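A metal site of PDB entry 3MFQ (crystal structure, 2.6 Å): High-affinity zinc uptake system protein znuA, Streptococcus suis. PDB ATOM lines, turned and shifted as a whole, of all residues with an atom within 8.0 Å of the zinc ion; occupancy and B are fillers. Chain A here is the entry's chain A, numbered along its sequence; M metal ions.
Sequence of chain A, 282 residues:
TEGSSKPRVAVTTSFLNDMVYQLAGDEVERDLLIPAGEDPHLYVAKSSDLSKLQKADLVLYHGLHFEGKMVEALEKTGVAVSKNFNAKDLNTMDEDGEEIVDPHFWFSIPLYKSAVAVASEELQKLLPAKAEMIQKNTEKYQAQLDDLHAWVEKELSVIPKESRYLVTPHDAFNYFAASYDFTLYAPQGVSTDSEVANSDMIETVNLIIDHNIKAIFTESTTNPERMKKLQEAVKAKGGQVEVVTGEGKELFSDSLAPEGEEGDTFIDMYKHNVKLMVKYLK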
ATOM      1  N   ASP A  39      -9.582 -18.756 -14.901  1.00  0.00           N
ATOM      2  CA  ASP A  39      -9.448 -17.933 -13.701  1.00  0.00           C
ATOM      3  C   ASP A  39      -9.238 -18.778 -12.454  1.00  0.00           C
ATOM      4  O   ASP A  39     -10.151 -19.453 -11.992  1.00  0.00           O
ATOM      5  CB  ASP A  39     -10.692 -17.065 -13.539  1.00  0.00           C
ATOM      6  CG  ASP A  39     -10.591 -16.123 -12.354  1.00  0.00           C
ATOM      7  OD1 ASP A  39      -9.628 -16.240 -11.573  1.00  0.00           O
ATOM      8  OD2 ASP A  39     -11.480 -15.256 -12.218  1.00  0.00           O
ATOM      9  N   PRO A  40      -8.024 -18.713 -11.887  1.00  0.00           N
ATOM     10  CA  PRO A  40      -7.666 -19.460 -10.672  1.00  0.00           C
ATOM     11  C   PRO A  40      -8.574 -19.111  -9.493  1.00  0.00           C
ATOM     12  O   PRO A  40      -8.777 -19.948  -8.623  1.00  0.00           O
ATOM     13  CB  PRO A  40      -6.227 -19.015 -10.396  1.00  0.00           C
ATOM     14  CG  PRO A  40      -5.709 -18.594 -11.731  1.00  0.00           C
ATOM     15  CD  PRO A  40      -6.871 -17.966 -12.424  1.00  0.00           C
ATOM     16  N   HIS A  41      -9.099 -17.886  -9.461  1.00  0.00           N
ATOM     17  CA  HIS A  41      -9.989 -17.476  -8.384  1.00  0.00           C
ATOM     18  C   HIS A  41     -11.170 -18.427  -8.263  1.00  0.00           C
ATOM     19  O   HIS A  41     -11.692 -18.649  -7.175  1.00  0.00           O
ATOM     20  CB  HIS A  41     -10.521 -16.062  -8.635  1.00  0.00           C
ATOM     21  CG  HIS A  41      -9.507 -14.978  -8.389  1.00  0.00           C
ATOM     22  ND1 HIS A  41      -9.011 -14.697  -7.134  1.00  0.00           N
ATOM     23  CD2 HIS A  41      -8.931 -14.101  -9.241  1.00  0.00           C
ATOM     24  CE1 HIS A  41      -8.155 -13.692  -7.223  1.00  0.00           C
ATOM     25  NE2 HIS A  41      -8.089 -13.314  -8.493  1.00  0.00           N
ATOM     26  N   PHE A  66      -4.845 -17.173  -4.015  1.00  0.00           N
ATOM     27  CA  PHE A  66      -5.036 -16.869  -5.435  1.00  0.00           C
ATOM     28  C   PHE A  66      -5.882 -17.956  -6.101  1.00  0.00           C
ATOM     29  O   PHE A  66      -6.903 -17.661  -6.727  1.00  0.00           O
ATOM     30  CB  PHE A  66      -3.682 -16.723  -6.139  1.00  0.00           C
ATOM     31  CG  PHE A  66      -3.784 -16.545  -7.628  1.00  0.00           C
ATOM     32  CD1 PHE A  66      -4.783 -15.747  -8.174  1.00  0.00           C
ATOM     33  CD2 PHE A  66      -2.881 -17.153  -8.475  1.00  0.00           C
ATOM     34  CE1 PHE A  66      -4.879 -15.578  -9.546  1.00  0.00           C
ATOM     35  CE2 PHE A  66      -2.976 -16.984  -9.847  1.00  0.00           C
ATOM     36  CZ  PHE A  66      -3.971 -16.196 -10.380  1.00  0.00           C
ATOM     37  N   ASP A 102      -3.977  -9.245  -1.009  1.00  0.00           N
ATOM     38  CA  ASP A 102      -4.049  -9.155  -2.460  1.00  0.00           C
ATOM     39  C   ASP A 102      -3.043 -10.128  -3.081  1.00  0.00           C
ATOM     40  O   ASP A 102      -1.832  -9.995  -2.876  1.00  0.00           O
ATOM     41  CB  ASP A 102      -3.766  -7.721  -2.923  1.00  0.00           C
ATOM     42  CG  ASP A 102      -3.917  -7.535  -4.426  1.00  0.00           C
ATOM     43  OD1 ASP A 102      -3.941  -8.551  -5.153  1.00  0.00           O
ATOM     44  OD2 ASP A 102      -4.001  -6.380  -4.875  1.00  0.00           O
ATOM     45  N   PRO A 103      -3.538 -11.118  -3.841  1.00  0.00           N
ATOM     46  CA  PRO A 103      -2.716 -12.200  -4.381  1.00  0.00           C
ATOM     47  C   PRO A 103      -1.891 -11.803  -5.610  1.00  0.00           C
ATOM     48  O   PRO A 103      -0.954 -12.517  -5.955  1.00  0.00           O
ATOM     49  CB  PRO A 103      -3.755 -13.256  -4.775  1.00  0.00           C
ATOM     50  CG  PRO A 103      -4.979 -12.469  -5.090  1.00  0.00           C
ATOM     51  CD  PRO A 103      -4.964 -11.282  -4.172  1.00  0.00           C
ATOM     52  N   HIS A 104      -2.237 -10.692  -6.244  1.00  0.00           N
ATOM     53  CA  HIS A 104      -1.607 -10.305  -7.509  1.00  0.00           C
ATOM     54  C   HIS A 104      -0.213  -9.712  -7.310  1.00  0.00           C
ATOM     55  O   HIS A 104       0.049  -8.589  -7.746  1.00  0.00           O
ATOM     56  CB  HIS A 104      -2.490  -9.312  -8.250  1.00  0.00           C
ATOM     57  CG  HIS A 104      -3.925  -9.746  -8.365  1.00  0.00           C
ATOM     58  ND1 HIS A 104      -4.896  -9.331  -7.478  1.00  0.00           N
ATOM     59  CD2 HIS A 104      -4.538 -10.563  -9.241  1.00  0.00           C
ATOM     60  CE1 HIS A 104      -6.056  -9.863  -7.823  1.00  0.00           C
ATOM     61  NE2 HIS A 104      -5.870 -10.619  -8.885  1.00  0.00           N
ATOM     62  N   TRP A 106       2.641 -10.674  -8.591  1.00  0.00           N
ATOM     63  CA  TRP A 106       3.574 -10.861  -9.708  1.00  0.00           C
ATOM     64  C   TRP A 106       3.866  -9.608 -10.532  1.00  0.00           C
ATOM     65  O   TRP A 106       4.832  -9.563 -11.287  1.00  0.00           O
ATOM     66  CB  TRP A 106       3.118 -12.010 -10.610  1.00  0.00           C
ATOM     67  CG  TRP A 106       1.685 -11.915 -11.018  1.00  0.00           C
ATOM     68  CD1 TRP A 106       1.181 -11.265 -12.097  1.00  0.00           C
ATOM     69  CD2 TRP A 106       0.565 -12.510 -10.346  1.00  0.00           C
ATOM     70  NE1 TRP A 106      -0.181 -11.405 -12.144  1.00  0.00           N
ATOM     71  CE2 TRP A 106      -0.585 -12.161 -11.074  1.00  0.00           C
ATOM     72  CE3 TRP A 106       0.429 -13.293  -9.201  1.00  0.00           C
ATOM     73  CZ2 TRP A 106      -1.855 -12.575 -10.693  1.00  0.00           C
ATOM     74  CZ3 TRP A 106      -0.827 -13.695  -8.825  1.00  0.00           C
ATOM     75  CH2 TRP A 106      -1.960 -13.336  -9.565  1.00  0.00           C
ATOM     76  N   PHE A 107       3.022  -8.580 -10.391  1.00  0.00           N
ATOM     77  CA  PHE A 107       3.257  -7.319 -11.087  1.00  0.00           C
ATOM     78  C   PHE A 107       4.259  -6.443 -10.331  1.00  0.00           C
ATOM     79  O   PHE A 107       4.736  -5.440 -10.860  1.00  0.00           O
ATOM     80  CB  PHE A 107       1.948  -6.576 -11.324  1.00  0.00           C
ATOM     81  CG  PHE A 107       1.039  -7.238 -12.320  1.00  0.00           C
ATOM     82  CD1 PHE A 107       1.434  -7.404 -13.642  1.00  0.00           C
ATOM     83  CD2 PHE A 107      -0.206  -7.700 -11.938  1.00  0.00           C
ATOM     84  CE1 PHE A 107       0.602  -8.021 -14.551  1.00  0.00           C
ATOM     85  CE2 PHE A 107      -1.047  -8.318 -12.852  1.00  0.00           C
ATOM     86  CZ  PHE A 107      -0.639  -8.473 -14.156  1.00  0.00           C
ATOM     87  N   HIS A 170     -11.280  -5.824 -12.306  1.00  0.00           N
ATOM     88  CA  HIS A 170     -11.147  -6.071 -10.871  1.00  0.00           C
ATOM     89  C   HIS A 170      -9.773  -5.678 -10.337  1.00  0.00           C
ATOM     90  O   HIS A 170      -8.829  -5.473 -11.088  1.00  0.00           O
ATOM     91  CB  HIS A 170     -11.493  -7.519 -10.521  1.00  0.00           C
ATOM     92  CG  HIS A 170     -10.405  -8.496 -10.826  1.00  0.00           C
ATOM     93  ND1 HIS A 170     -10.089  -8.897 -12.105  1.00  0.00           N
ATOM     94  CD2 HIS A 170      -9.571  -9.191 -10.002  1.00  0.00           C
ATOM     95  CE1 HIS A 170      -9.108  -9.778 -12.069  1.00  0.00           C
ATOM     96  NE2 HIS A 170      -8.772  -9.965 -10.807  1.00  0.00           N
ATOM     97  N   ASP A 171      -9.682  -5.567  -9.006  1.00  0.00           N
ATOM     98  CA  ASP A 171      -8.478  -5.092  -8.356  1.00  0.00           C
ATOM     99  C   ASP A 171      -7.335  -6.096  -8.462  1.00  0.00           C
ATOM    100  O   ASP A 171      -7.182  -6.965  -7.597  1.00  0.00           O
ATOM    101  CB  ASP A 171      -8.775  -4.800  -6.888  1.00  0.00           C
ATOM    102  CG  ASP A 171      -7.989  -3.616  -6.353  1.00  0.00           C
ATOM    103  OD1 ASP A 171      -6.994  -3.228  -7.005  1.00  0.00           O
ATOM    104  OD2 ASP A 171      -8.365  -3.090  -5.295  1.00  0.00           O
ATOM    105  N   ALA A 172      -6.536  -5.980  -9.507  1.00  0.00           N
ATOM    106  CA  ALA A 172      -5.476  -6.948  -9.760  1.00  0.00           C
ATOM    107  C   ALA A 172      -4.141  -6.280 -10.077  1.00  0.00           C
ATOM    108  O   ALA A 172      -3.162  -6.963 -10.377  1.00  0.00           O
ATOM    109  CB  ALA A 172      -5.880  -7.885 -10.889  1.00  0.00           C
ATOM    110  N   PHE A 173      -4.103  -4.956 -10.005  1.00  0.00           N
ATOM    111  CA  PHE A 173      -2.896  -4.216 -10.366  1.00  0.00           C
ATOM    112  C   PHE A 173      -2.429  -3.295  -9.248  1.00  0.00           C
ATOM    113  O   PHE A 173      -1.743  -2.300  -9.507  1.00  0.00           O
ATOM    114  CB  PHE A 173      -3.120  -3.412 -11.645  1.00  0.00           C
ATOM    115  CG  PHE A 173      -3.450  -4.265 -12.836  1.00  0.00           C
ATOM    116  CD1 PHE A 173      -4.771  -4.544 -13.159  1.00  0.00           C
ATOM    117  CD2 PHE A 173      -2.449  -4.778 -13.641  1.00  0.00           C
ATOM    118  CE1 PHE A 173      -5.080  -5.316 -14.269  1.00  0.00           C
ATOM    119  CE2 PHE A 173      -2.749  -5.560 -14.746  1.00  0.00           C
ATOM    120  CZ  PHE A 173      -4.067  -5.829 -15.056  1.00  0.00           C
ATOM    121  N   GLN A 188     -14.683  -4.181  -9.105  1.00  0.00           N
ATOM    122  CA  GLN A 188     -14.672  -5.398  -8.300  1.00  0.00           C
ATOM    123  C   GLN A 188     -13.488  -5.454  -7.344  1.00  0.00           C
ATOM    124  O   GLN A 188     -12.483  -4.763  -7.553  1.00  0.00           O
ATOM    125  CB  GLN A 188     -14.667  -6.634  -9.208  1.00  0.00           C
ATOM    126  CG  GLN A 188     -14.708  -7.944  -8.444  1.00  0.00           C
ATOM    127  CD  GLN A 188     -15.060  -9.128  -9.326  1.00  0.00           C
ATOM    128  OE1 GLN A 188     -15.905  -9.940  -8.978  1.00  0.00           O
ATOM    129  NE2 GLN A 188     -14.409  -9.210 -10.477  1.00  0.00           N
ATOM    130  N   GLY A 189     -13.611  -6.266  -6.306  1.00  0.00           N
ATOM    131  CA  GLY A 189     -12.573  -6.369  -5.305  1.00  0.00           C
ATOM    132  C   GLY A 189     -11.325  -7.078  -5.790  1.00  0.00           C
ATOM    133  O   GLY A 189     -11.021  -7.088  -6.977  1.00  0.00           O
ATOM    134  N   VAL A 190     -10.592  -7.668  -4.848  1.00  0.00           N
ATOM    135  CA  VAL A 190      -9.340  -8.356  -5.150  1.00  0.00           C
ATOM    136  C   VAL A 190      -9.590  -9.713  -5.800  1.00  0.00           C
ATOM    137  O   VAL A 190      -8.884 -10.102  -6.725  1.00  0.00           O
ATOM    138  CB  VAL A 190      -8.490  -8.517  -3.876  1.00  0.00           C
ATOM    139  CG1 VAL A 190      -8.093  -9.968  -3.686  1.00  0.00           C
ATOM    140  CG2 VAL A 190      -7.270  -7.624  -3.955  1.00  0.00           C
ATOM    141  N   SER A 191     -10.605 -10.424  -5.314  1.00  0.00           N
ATOM    142  CA  SER A 191     -10.991 -11.688  -5.910  1.00  0.00           C
ATOM    143  C   SER A 191     -12.066 -11.457  -6.962  1.00  0.00           C
ATOM    144  O   SER A 191     -12.741 -10.430  -6.946  1.00  0.00           O
ATOM    145  CB  SER A 191     -11.511 -12.651  -4.837  1.00  0.00           C
ATOM    146  OG  SER A 191     -11.963 -13.868  -5.421  1.00  0.00           O
ATOM    147  N   THR A 192     -12.210 -12.400  -7.875  1.00  0.00           N
ATOM    148  CA  THR A 192     -13.233 -12.297  -8.903  1.00  0.00           C
ATOM    149  C   THR A 192     -14.446 -13.128  -8.501  1.00  0.00           C
ATOM    150  O   THR A 192     -15.411 -13.251  -9.254  1.00  0.00           O
ATOM    151  CB  THR A 192     -12.730 -12.798 -10.266  1.00  0.00           C
ATOM    152  OG1 THR A 192     -12.613 -14.224 -10.236  1.00  0.00           O
ATOM    153  CG2 THR A 192     -11.378 -12.180 -10.588  1.00  0.00           C
ATOM    154  N   ASP A 193     -14.383 -13.710  -7.303  1.00  0.00           N
ATOM    155  CA  ASP A 193     -15.449 -14.563  -6.813  1.00  0.00           C
ATOM    156  C   ASP A 193     -16.473 -13.761  -6.013  1.00  0.00           C
ATOM    157  O   ASP A 193     -16.580 -13.921  -4.794  1.00  0.00           O
ATOM    158  CB  ASP A 193     -14.879 -15.702  -5.958  1.00  0.00           C
ATOM    159  CG  ASP A 193     -15.902 -16.774  -5.654  1.00  0.00           C
ATOM    160  OD1 ASP A 193     -17.046 -16.675  -6.157  1.00  0.00           O
ATOM    161  OD2 ASP A 193     -15.567 -17.725  -4.908  1.00  0.00           O
ATOM    162  N   GLU A 219      -9.760  -7.242 -19.560  1.00  0.00           N
ATOM    163  CA  GLU A 219      -8.863  -8.356 -19.279  1.00  0.00           C
ATOM    164  C   GLU A 219      -9.399  -9.668 -19.865  1.00  0.00           C
ATOM    165  O   GLU A 219     -10.596  -9.820 -20.074  1.00  0.00           O
ATOM    166  CB  GLU A 219      -8.646  -8.508 -17.774  1.00  0.00           C
ATOM    167  CG  GLU A 219      -9.889  -8.919 -17.017  1.00  0.00           C
ATOM    168  CD  GLU A 219      -9.728  -8.774 -15.524  1.00  0.00           C
ATOM    169  OE1 GLU A 219      -8.641  -8.346 -15.073  1.00  0.00           O
ATOM    170  OE2 GLU A 219     -10.688  -9.090 -14.795  1.00  0.00           O
ATOM    171  N   THR A 221      -9.465 -12.740 -18.644  1.00  0.00           N
ATOM    172  CA  THR A 221     -10.054 -13.737 -17.757  1.00  0.00           C
ATOM    173  C   THR A 221     -11.487 -13.448 -17.310  1.00  0.00           C
ATOM    174  O   THR A 221     -12.159 -14.321 -16.770  1.00  0.00           O
ATOM    175  CB  THR A 221      -9.159 -13.986 -16.517  1.00  0.00           C
ATOM    176  OG1 THR A 221      -8.541 -12.761 -16.116  1.00  0.00           O
ATOM    177  CG2 THR A 221      -8.086 -15.014 -16.831  1.00  0.00           C
ATOM    178  N   THR A 222     -11.964 -12.232 -17.559  1.00  0.00           N
ATOM    179  CA  THR A 222     -13.352 -11.890 -17.201  1.00  0.00           C
ATOM    180  C   THR A 222     -14.156 -11.366 -18.386  1.00  0.00           C
ATOM    181  O   THR A 222     -13.599 -10.972 -19.407  1.00  0.00           O
ATOM    182  CB  THR A 222     -13.421 -10.847 -16.048  1.00  0.00           C
ATOM    183  OG1 THR A 222     -12.756  -9.643 -16.438  1.00  0.00           O
ATOM    184  CG2 THR A 222     -12.779 -11.399 -14.791  1.00  0.00           C
ATOM    185  N   SER A 253      -4.291 -10.392 -16.308  1.00  0.00           N
ATOM    186  CA  SER A 253      -4.192 -10.210 -14.870  1.00  0.00           C
ATOM    187  C   SER A 253      -3.980 -11.548 -14.176  1.00  0.00           C
ATOM    188  O   SER A 253      -3.027 -11.716 -13.413  1.00  0.00           O
ATOM    189  CB  SER A 253      -5.450  -9.531 -14.322  1.00  0.00           C
ATOM    190  OG  SER A 253      -6.546 -10.428 -14.325  1.00  0.00           O
ATOM    191  N   ASP A 254      -4.874 -12.496 -14.446  1.00  0.00           N
ATOM    192  CA  ASP A 254      -4.863 -13.764 -13.743  1.00  0.00           C
ATOM    193  C   ASP A 254      -4.401 -14.916 -14.623  1.00  0.00           C
ATOM    194  O   ASP A 254      -4.645 -16.078 -14.303  1.00  0.00           O
ATOM    195  CB  ASP A 254      -6.254 -14.073 -13.187  1.00  0.00           C
ATOM    196  CG  ASP A 254      -6.676 -13.078 -12.131  1.00  0.00           C
ATOM    197  OD1 ASP A 254      -5.793 -12.400 -11.557  1.00  0.00           O
ATOM    198  OD2 ASP A 254      -7.889 -12.959 -11.867  1.00  0.00           O
ATOM    199  N   SER A 255      -3.722 -14.606 -15.716  1.00  0.00           N
ATOM    200  CA  SER A 255      -3.235 -15.636 -16.613  1.00  0.00           C
ATOM    201  C   SER A 255      -2.349 -15.085 -17.716  1.00  0.00           C
ATOM    202  O   SER A 255      -2.496 -13.943 -18.130  1.00  0.00           O
ATOM    203  CB  SER A 255      -4.422 -16.381 -17.249  1.00  0.00           C
ATOM    204  OG  SER A 255      -3.968 -17.343 -18.196  1.00  0.00           O
HETATM  205 ZN    ZN M   1      -7.452 -11.516 -10.062  1.00  0.00          ZN
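A ring nitrogen (ND1) of His 104 sits close to the backbone carbonyl oxygen of Asp 171 (3.3 Å).
A ring nitrogen (ND1) of His 104 sits at hydrogen-bond distance from the side-chain carboxylate (OD1) of Asp 102.
The side-chain carboxylate of Glu 219 is in hydrogen-bond range of a ring nitrogen (ND1) of His 170, 2.8 Å away.
OD1 of Asp 254 sits close to OG of Ser 253.
The side-chain carboxylate (OD1) of Asp 39 sits at hydrogen-bond distance from the backbone NH (N) of His 41 (2.7 Å).
Val 190 touches the zinc ion (O to ZN, 3.9 Å).
The nearest printed residue that does not touch the zinc ion is Thr 192 (4.02 Å).
The zinc ion is bound by NE2 of His 104 (2.2 Å), NE2 of His 170 (2.2 Å), OD2 of Asp 254 (2.4 Å), OD1 of Asp 254 (2.4 Å) and NE2 of His 41 (2.5 Å).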
